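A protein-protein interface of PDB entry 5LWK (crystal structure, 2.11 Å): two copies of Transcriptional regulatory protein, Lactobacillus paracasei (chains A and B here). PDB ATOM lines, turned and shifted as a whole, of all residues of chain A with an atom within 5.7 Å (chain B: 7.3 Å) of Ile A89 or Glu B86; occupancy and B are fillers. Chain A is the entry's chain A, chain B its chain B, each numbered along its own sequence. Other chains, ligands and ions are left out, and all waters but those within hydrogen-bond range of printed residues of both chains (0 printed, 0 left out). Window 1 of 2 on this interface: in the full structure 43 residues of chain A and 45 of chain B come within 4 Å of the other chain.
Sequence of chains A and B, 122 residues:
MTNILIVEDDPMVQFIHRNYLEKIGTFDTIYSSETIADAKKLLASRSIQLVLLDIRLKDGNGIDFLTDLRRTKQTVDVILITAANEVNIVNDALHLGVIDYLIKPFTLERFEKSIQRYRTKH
The backbone carbonyl oxygen (O) of Ala A84 lies within hydrogen-bond range of the side-chain hydroxyl (OH) of Tyr B101 (2.9 Å). The side-chain carboxylate (OE2) of Glu A86 sits close to the side-chain carboxylate (OE2) of Glu B86 (3.4 Å).
OD1 of Asn A85 sits close to N of Val A87 (3.4 Å). The side-chain amide oxygen (OD1) of Asn A85 lies within hydrogen-bond range of the side-chain amide nitrogen (ND2) of Asn A88, at 2.9 Å. O of Ile A89 is in hydrogen-bond range of N of Leu A94. N of Val B87 sits close to OD1 of Asn B85 (3.2 Å). The backbone NH (N) of Asn B88 sits at hydrogen-bond distance from the side-chain amide oxygen (OD1) of Asn B85. O of Ile B89 is in hydrogen-bond range of N of Leu B94 (2.9 Å).
Among the printed residues, pairs that only touch across the chains: Ile A55 with Tyr B101 (3.8 Å), Ala A84 with Glu B86 (3.9 Å), Asn A85 with Glu B86 (3.4 Å), Glu A86 with Ala B84 (3.8 Å), Glu A86 with Asn B85 (3.4 Å), Glu A86 with Ile B89 (3.96 Å), Ile A89 with Glu B86 (3.97 Å) and Ile A89 with Tyr B101 (3.6 Å).
Of the printed residues of chain B, Ile A55 touches Tyr B101 (3.8 Å). Printed residues of chain B within 4 Å of Glu A86: Ala B84 (3.8 Å), Asn B85 (3.4 Å), Glu B86 (3.4 Å) and Ile B89 (3.96 Å). Of chain B, only Glu B86 (3.97 Å) and Tyr B101 (3.6 Å) come within 4 Å of Ile A89. Glu B86 touches four residues of chain A. Asp B92 touches none of the printed residues of chain A. Val B98 touches none of the printed residues of chain A. The nearest printed residue of chain A that does not touch Glu B86 is Val A87 (6.4 Å). The nearest printed residue of chain B that does not touch Glu A86 is Tyr B101 (5.9 Å).
Of the 14 printed residues of chain B, 5 touch a printed residue of chain A. Hydrophobic or aromatic side chains of chain B that line the printed part of chain A: Ile B89 and Tyr B101. Along chain B the printed residues that touch a printed residue of chain A span positions 84 to 101. Among the printed residues, no Asp or Glu carboxylate lies within 4 Å of a Lys or Arg side-chain nitrogen of the other chain.
Ala A84 touches Glu B86, and with the chains exchanged Glu A86 touches Ala B84. Asn A85 touches Glu B86, and with the chains exchanged Glu A86 touches Asn B85. Glu A86 touches its own counterpart, Glu B86. Glu A86 touches Ile B89, and with the chains exchanged Ile A89 touches Glu B86. 10 positions are printed for both chains. Of the 10 pairs that touch across the chains among the printed residues, 7 have their exchanged pair printed and touching as well.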
ATOM      1  N   ILE A  55      24.597  -4.824  15.271  1.00  0.00           N
ATOM      2  CA  ILE A  55      24.353  -6.182  15.813  1.00  0.00           C
ATOM      3  C   ILE A  55      24.694  -6.302  17.301  1.00  0.00           C
ATOM      4  O   ILE A  55      23.851  -6.752  18.083  1.00  0.00           O
ATOM      5  CB  ILE A  55      25.054  -7.284  14.991  1.00  0.00           C
ATOM      6  CG1 ILE A  55      24.381  -7.393  13.620  1.00  0.00           C
ATOM      7  CG2 ILE A  55      24.992  -8.629  15.711  1.00  0.00           C
ATOM      8  CD1 ILE A  55      25.017  -8.383  12.668  1.00  0.00           C
ATOM      9  N   ILE A  63      20.449  -9.289  15.495  1.00  0.00           N
ATOM     10  CA  ILE A  63      19.838 -10.335  14.655  1.00  0.00           C
ATOM     11  C   ILE A  63      18.560 -10.896  15.277  1.00  0.00           C
ATOM     12  O   ILE A  63      17.599 -11.157  14.554  1.00  0.00           O
ATOM     13  CB  ILE A  63      20.806 -11.493  14.338  1.00  0.00           C
ATOM     14  CG1 ILE A  63      22.052 -10.976  13.605  1.00  0.00           C
ATOM     15  CG2 ILE A  63      20.120 -12.579  13.503  1.00  0.00           C
ATOM     16  CD1 ILE A  63      21.799 -10.254  12.294  1.00  0.00           C
ATOM     17  N   ALA A  84      30.305  -7.151  12.535  1.00  0.00           N
ATOM     18  CA  ALA A  84      30.185  -8.592  12.446  1.00  0.00           C
ATOM     19  C   ALA A  84      30.474  -9.234  11.108  1.00  0.00           C
ATOM     20  O   ALA A  84      30.021  -8.805  10.092  1.00  0.00           O
ATOM     21  CB  ALA A  84      28.830  -9.015  12.932  1.00  0.00           C
ATOM     22  N   ASN A  85      31.249 -10.295  11.152  1.00  0.00           N
ATOM     23  CA  ASN A  85      31.585 -11.083   9.992  1.00  0.00           C
ATOM     24  C   ASN A  85      30.751 -12.353  10.042  1.00  0.00           C
ATOM     25  O   ASN A  85      29.915 -12.485  10.894  1.00  0.00           O
ATOM     26  CB  ASN A  85      33.080 -11.325   9.848  1.00  0.00           C
ATOM     27  CG  ASN A  85      33.641 -12.195  10.920  1.00  0.00           C
ATOM     28  OD1 ASN A  85      32.942 -12.697  11.743  1.00  0.00           O
ATOM     29  ND2 ASN A  85      34.926 -12.356  10.907  1.00  0.00           N
ATOM     30  N   GLU A  86      30.963 -13.271   9.122  1.00  0.00           N
ATOM     31  CA  GLU A  86      30.155 -14.462   9.069  1.00  0.00           C
ATOM     32  C   GLU A  86      30.203 -15.306  10.310  1.00  0.00           C
ATOM     33  O   GLU A  86      29.198 -15.714  10.797  1.00  0.00           O
ATOM     34  CB  GLU A  86      30.603 -15.318   7.904  1.00  0.00           C
ATOM     35  CG  GLU A  86      30.465 -14.666   6.558  1.00  0.00           C
ATOM     36  CD  GLU A  86      31.699 -13.935   6.139  1.00  0.00           C
ATOM     37  OE1 GLU A  86      32.634 -13.831   6.915  1.00  0.00           O
ATOM     38  OE2 GLU A  86      31.722 -13.458   5.028  1.00  0.00           O
ATOM     39  N   VAL A  87      31.385 -15.535  10.826  1.00  0.00           N
ATOM     40  CA  VAL A  87      31.532 -16.332  12.006  1.00  0.00           C
ATOM     41  C   VAL A  87      30.878 -15.685  13.220  1.00  0.00           C
ATOM     42  O   VAL A  87      30.356 -16.360  14.055  1.00  0.00           O
ATOM     43  CB  VAL A  87      32.963 -16.855  12.205  1.00  0.00           C
ATOM     44  CG1 VAL A  87      33.903 -15.782  12.673  1.00  0.00           C
ATOM     45  CG2 VAL A  87      32.964 -18.040  13.128  1.00  0.00           C
ATOM     46  N   ASN A  88      30.930 -14.368  13.302  1.00  0.00           N
ATOM     47  CA  ASN A  88      30.320 -13.665  14.392  1.00  0.00           C
ATOM     48  C   ASN A  88      28.812 -13.918  14.356  1.00  0.00           C
ATOM     49  O   ASN A  88      28.214 -14.125  15.365  1.00  0.00           O
ATOM     50  CB  ASN A  88      30.603 -12.167  14.319  1.00  0.00           C
ATOM     51  CG  ASN A  88      32.060 -11.822  14.491  1.00  0.00           C
ATOM     52  OD1 ASN A  88      32.781 -12.482  15.194  1.00  0.00           O
ATOM     53  ND2 ASN A  88      32.475 -10.763  13.868  1.00  0.00           N
ATOM     54  N   ILE A  89      28.210 -13.897  13.185  1.00  0.00           N
ATOM     55  CA  ILE A  89      26.792 -14.163  13.077  1.00  0.00           C
ATOM     56  C   ILE A  89      26.442 -15.584  13.465  1.00  0.00           C
ATOM     57  O   ILE A  89      25.593 -15.797  14.261  1.00  0.00           O
ATOM     58  CB  ILE A  89      26.303 -13.952  11.640  1.00  0.00           C
ATOM     59  CG1 ILE A  89      26.535 -12.522  11.220  1.00  0.00           C
ATOM     60  CG2 ILE A  89      24.840 -14.309  11.492  1.00  0.00           C
ATOM     61  CD1 ILE A  89      26.195 -12.264   9.788  1.00  0.00           C
ATOM     62  N   VAL A  90      27.157 -16.534  12.919  1.00  0.00           N
ATOM     63  CA  VAL A  90      26.924 -17.949  13.189  1.00  0.00           C
ATOM     64  C   VAL A  90      27.092 -18.292  14.688  1.00  0.00           C
ATOM     65  O   VAL A  90      26.252 -18.985  15.266  1.00  0.00           O
ATOM     66  CB  VAL A  90      27.826 -18.830  12.284  1.00  0.00           C
ATOM     67  CG1 VAL A  90      27.816 -20.294  12.708  1.00  0.00           C
ATOM     68  CG2 VAL A  90      27.364 -18.724  10.834  1.00  0.00           C
ATOM     69  N   ASN A  91      28.149 -17.780  15.311  1.00  0.00           N
ATOM     70  CA  ASN A  91      28.477 -18.156  16.691  1.00  0.00           C
ATOM     71  C   ASN A  91      27.913 -17.218  17.740  1.00  0.00           C
ATOM     72  O   ASN A  91      27.431 -17.693  18.763  1.00  0.00           O
ATOM     73  CB  ASN A  91      29.997 -18.313  16.881  1.00  0.00           C
ATOM     74  CG  ASN A  91      30.513 -19.641  16.356  1.00  0.00           C
ATOM     75  OD1 ASN A  91      29.733 -20.530  16.001  1.00  0.00           O
ATOM     76  ND2 ASN A  91      31.831 -19.791  16.309  1.00  0.00           N
ATOM     77  N   ASP A  92      27.978 -15.905  17.515  1.00  0.00           N
ATOM     78  CA  ASP A  92      27.559 -14.943  18.553  1.00  0.00           C
ATOM     79  C   ASP A  92      26.098 -14.498  18.446  1.00  0.00           C
ATOM     80  O   ASP A  92      25.492 -14.132  19.453  1.00  0.00           O
ATOM     81  CB  ASP A  92      28.509 -13.746  18.602  1.00  0.00           C
ATOM     82  CG  ASP A  92      29.965 -14.167  18.809  1.00  0.00           C
ATOM     83  OD1 ASP A  92      30.215 -15.220  19.432  1.00  0.00           O
ATOM     84  OD2 ASP A  92      30.868 -13.453  18.351  1.00  0.00           O
ATOM     85  N   ALA A  93      25.526 -14.538  17.246  1.00  0.00           N
ATOM     86  CA  ALA A  93      24.101 -14.230  17.072  1.00  0.00           C
ATOM     87  C   ALA A  93      23.254 -15.497  17.110  1.00  0.00           C
ATOM     88  O   ALA A  93      22.241 -15.541  17.792  1.00  0.00           O
ATOM     89  CB  ALA A  93      23.867 -13.466  15.780  1.00  0.00           C
ATOM     90  N   LEU A  94      23.666 -16.522  16.371  1.00  0.00           N
ATOM     91  CA  LEU A  94      22.909 -17.773  16.314  1.00  0.00           C
ATOM     92  C   LEU A  94      23.245 -18.784  17.410  1.00  0.00           C
ATOM     93  O   LEU A  94      22.408 -19.610  17.773  1.00  0.00           O
ATOM     94  CB  LEU A  94      23.073 -18.427  14.938  1.00  0.00           C
ATOM     95  CG  LEU A  94      22.100 -17.967  13.850  1.00  0.00           C
ATOM     96  CD1 LEU A  94      21.731 -16.505  14.042  1.00  0.00           C
ATOM     97  CD2 LEU A  94      22.692 -18.199  12.468  1.00  0.00           C
ATOM     98  N   HIS A  95      24.458 -18.715  17.929  1.00  0.00           N
ATOM     99  CA  HIS A  95      24.912 -19.644  18.940  1.00  0.00           C
ATOM    100  C   HIS A  95      25.101 -21.051  18.421  1.00  0.00           C
ATOM    101  O   HIS A  95      24.851 -21.996  19.107  1.00  0.00           O
ATOM    102  CB  HIS A  95      23.945 -19.669  20.111  1.00  0.00           C
ATOM    103  CG  HIS A  95      23.589 -18.324  20.624  1.00  0.00           C
ATOM    104  ND1 HIS A  95      24.530 -17.413  21.021  1.00  0.00           N
ATOM    105  CD2 HIS A  95      22.391 -17.733  20.802  1.00  0.00           C
ATOM    106  CE1 HIS A  95      23.928 -16.317  21.421  1.00  0.00           C
ATOM    107  NE2 HIS A  95      22.630 -16.488  21.300  1.00  0.00           N
ATOM    108  N   ALA B  83      30.806 -20.384   0.206  1.00  0.00           N
ATOM    109  CA  ALA B  83      30.949 -19.154  -0.502  1.00  0.00           C
ATOM    110  C   ALA B  83      30.106 -18.049   0.103  1.00  0.00           C
ATOM    111  O   ALA B  83      30.220 -16.929  -0.284  1.00  0.00           O
ATOM    112  CB  ALA B  83      30.578 -19.350  -1.951  1.00  0.00           C
ATOM    113  N   ALA B  84      29.256 -18.380   1.049  1.00  0.00           N
ATOM    114  CA  ALA B  84      28.381 -17.390   1.642  1.00  0.00           C
ATOM    115  C   ALA B  84      29.032 -16.289   2.465  1.00  0.00           C
ATOM    116  O   ALA B  84      29.851 -16.545   3.293  1.00  0.00           O
ATOM    117  CB  ALA B  84      27.319 -18.070   2.463  1.00  0.00           C
ATOM    118  N   ASN B  85      28.613 -15.067   2.210  1.00  0.00           N
ATOM    119  CA  ASN B  85      29.046 -13.897   2.925  1.00  0.00           C
ATOM    120  C   ASN B  85      27.948 -13.538   3.908  1.00  0.00           C
ATOM    121  O   ASN B  85      26.987 -14.229   4.006  1.00  0.00           O
ATOM    122  CB  ASN B  85      29.393 -12.746   1.999  1.00  0.00           C
ATOM    123  CG  ASN B  85      28.222 -12.257   1.212  1.00  0.00           C
ATOM    124  OD1 ASN B  85      27.106 -12.432   1.590  1.00  0.00           O
ATOM    125  ND2 ASN B  85      28.486 -11.637   0.112  1.00  0.00           N
ATOM    126  N   GLU B  86      28.117 -12.460   4.643  1.00  0.00           N
ATOM    127  CA  GLU B  86      27.166 -12.088   5.659  1.00  0.00           C
ATOM    128  C   GLU B  86      25.770 -11.854   5.164  1.00  0.00           C
ATOM    129  O   GLU B  86      24.843 -12.320   5.758  1.00  0.00           O
ATOM    130  CB  GLU B  86      27.635 -10.831   6.373  1.00  0.00           C
ATOM    131  CG  GLU B  86      28.979 -10.932   7.056  1.00  0.00           C
ATOM    132  CD  GLU B  86      30.142 -10.550   6.177  1.00  0.00           C
ATOM    133  OE1 GLU B  86      29.972 -10.296   5.000  1.00  0.00           O
ATOM    134  OE2 GLU B  86      31.246 -10.495   6.683  1.00  0.00           O
ATOM    135  N   VAL B  87      25.639 -11.135   4.072  1.00  0.00           N
ATOM    136  CA  VAL B  87      24.343 -10.862   3.500  1.00  0.00           C
ATOM    137  C   VAL B  87      23.665 -12.142   3.012  1.00  0.00           C
ATOM    138  O   VAL B  87      22.476 -12.302   3.119  1.00  0.00           O
ATOM    139  CB  VAL B  87      24.355  -9.673   2.535  1.00  0.00           C
ATOM    140  CG1 VAL B  87      25.229  -9.911   1.347  1.00  0.00           C
ATOM    141  CG2 VAL B  87      22.959  -9.293   2.148  1.00  0.00           C
ATOM    142  N   ASN B  88      24.466 -13.051   2.496  1.00  0.00           N
ATOM    143  CA  ASN B  88      23.979 -14.326   2.044  1.00  0.00           C
ATOM    144  C   ASN B  88      23.366 -15.051   3.224  1.00  0.00           C
ATOM    145  O   ASN B  88      22.361 -15.661   3.082  1.00  0.00           O
ATOM    146  CB  ASN B  88      25.102 -15.184   1.470  1.00  0.00           C
ATOM    147  CG  ASN B  88      25.608 -14.693   0.134  1.00  0.00           C
ATOM    148  OD1 ASN B  88      24.906 -14.050  -0.606  1.00  0.00           O
ATOM    149  ND2 ASN B  88      26.824 -15.005  -0.167  1.00  0.00           N
ATOM    150  N   ILE B  89      23.997 -14.998   4.381  1.00  0.00           N
ATOM    151  CA  ILE B  89      23.442 -15.630   5.549  1.00  0.00           C
ATOM    152  C   ILE B  89      22.173 -14.942   6.057  1.00  0.00           C
ATOM    153  O   ILE B  89      21.212 -15.566   6.351  1.00  0.00           O
ATOM    154  CB  ILE B  89      24.463 -15.697   6.697  1.00  0.00           C
ATOM    155  CG1 ILE B  89      25.637 -16.576   6.330  1.00  0.00           C
ATOM    156  CG2 ILE B  89      23.841 -16.265   7.947  1.00  0.00           C
ATOM    157  CD1 ILE B  89      26.851 -16.325   7.158  1.00  0.00           C
ATOM    158  N   VAL B  90      22.203 -13.636   6.140  1.00  0.00           N
ATOM    159  CA  VAL B  90      21.085 -12.881   6.694  1.00  0.00           C
ATOM    160  C   VAL B  90      19.831 -13.006   5.811  1.00  0.00           C
ATOM    161  O   VAL B  90      18.735 -13.201   6.331  1.00  0.00           O
ATOM    162  CB  VAL B  90      21.467 -11.396   6.926  1.00  0.00           C
ATOM    163  CG1 VAL B  90      20.256 -10.552   7.304  1.00  0.00           C
ATOM    164  CG2 VAL B  90      22.518 -11.279   8.026  1.00  0.00           C
ATOM    165  N   ASN B  91      20.005 -12.897   4.494  1.00  0.00           N
ATOM    166  CA  ASN B  91      18.883 -12.904   3.553  1.00  0.00           C
ATOM    167  C   ASN B  91      18.551 -14.284   2.986  1.00  0.00           C
ATOM    168  O   ASN B  91      17.386 -14.656   2.950  1.00  0.00           O
ATOM    169  CB  ASN B  91      19.127 -11.910   2.405  1.00  0.00           C
ATOM    170  CG  ASN B  91      18.895 -10.469   2.823  1.00  0.00           C
ATOM    171  OD1 ASN B  91      18.433 -10.192   3.935  1.00  0.00           O
ATOM    172  ND2 ASN B  91      19.200  -9.543   1.933  1.00  0.00           N
ATOM    173  N   ASP B  92      19.555 -15.041   2.556  1.00  0.00           N
ATOM    174  CA  ASP B  92      19.297 -16.338   1.910  1.00  0.00           C
ATOM    175  C   ASP B  92      19.126 -17.505   2.896  1.00  0.00           C
ATOM    176  O   ASP B  92      18.327 -18.408   2.637  1.00  0.00           O
ATOM    177  CB  ASP B  92      20.363 -16.660   0.863  1.00  0.00           C
ATOM    178  CG  ASP B  92      20.571 -15.525  -0.132  1.00  0.00           C
ATOM    179  OD1 ASP B  92      19.672 -14.671  -0.282  1.00  0.00           O
ATOM    180  OD2 ASP B  92      21.646 -15.482  -0.763  1.00  0.00           O
ATOM    181  N   LEU B  94      18.642 -16.992   6.581  1.00  0.00           N
ATOM    182  CA  LEU B  94      17.663 -16.559   7.580  1.00  0.00           C
ATOM    183  C   LEU B  94      16.350 -16.014   7.021  1.00  0.00           C
ATOM    184  O   LEU B  94      15.302 -16.130   7.657  1.00  0.00           O
ATOM    185  CB  LEU B  94      18.291 -15.526   8.521  1.00  0.00           C
ATOM    186  CG  LEU B  94      19.093 -16.082   9.699  1.00  0.00           C
ATOM    187  CD1 LEU B  94      19.772 -17.389   9.317  1.00  0.00           C
ATOM    188  CD2 LEU B  94      20.114 -15.064  10.183  1.00  0.00           C
ATOM    189  N   VAL B  98      17.047  -7.841   4.563  1.00  0.00           N
ATOM    190  CA  VAL B  98      17.657  -6.561   4.781  1.00  0.00           C
ATOM    191  C   VAL B  98      17.992  -5.928   3.457  1.00  0.00           C
ATOM    192  O   VAL B  98      18.290  -6.603   2.515  1.00  0.00           O
ATOM    193  CB  VAL B  98      18.919  -6.632   5.646  1.00  0.00           C
ATOM    194  CG1 VAL B  98      18.603  -7.181   7.008  1.00  0.00           C
ATOM    195  CG2 VAL B  98      20.010  -7.413   4.966  1.00  0.00           C
ATOM    196  N   TYR B 101      23.985  -4.758   3.779  1.00  0.00           N
ATOM    197  CA  TYR B 101      24.783  -5.100   4.924  1.00  0.00           C
ATOM    198  C   TYR B 101      26.095  -4.356   4.827  1.00  0.00           C
ATOM    199  O   TYR B 101      26.919  -4.706   4.031  1.00  0.00           O
ATOM    200  CB  TYR B 101      25.012  -6.602   4.946  1.00  0.00           C
ATOM    201  CG  TYR B 101      25.606  -7.170   6.200  1.00  0.00           C
ATOM    202  CD1 TYR B 101      26.937  -7.025   6.487  1.00  0.00           C
ATOM    203  CD2 TYR B 101      24.848  -7.891   7.064  1.00  0.00           C
ATOM    204  CE1 TYR B 101      27.478  -7.555   7.622  1.00  0.00           C
ATOM    205  CE2 TYR B 101      25.384  -8.421   8.197  1.00  0.00           C
ATOM    206  CZ  TYR B 101      26.699  -8.251   8.458  1.00  0.00           C
ATOM    207  OH  TYR B 101      27.217  -8.779   9.568  1.00  0.00           O
ATOM    208  N   ILE B 103      29.632  -3.416   6.354  1.00  0.00           N
ATOM    209  CA  ILE B 103      30.662  -3.828   7.282  1.00  0.00           C
ATOM    210  C   ILE B 103      31.386  -2.557   7.728  1.00  0.00           C
ATOM    211  O   ILE B 103      31.771  -1.729   6.894  1.00  0.00           O
ATOM    212  CB  ILE B 103      31.640  -4.820   6.620  1.00  0.00           C
ATOM    213  CG1 ILE B 103      30.882  -6.057   6.120  1.00  0.00           C
ATOM    214  CG2 ILE B 103      32.710  -5.267   7.605  1.00  0.00           C
ATOM    215  CD1 ILE B 103      31.577  -6.788   4.995  1.00  0.00           C
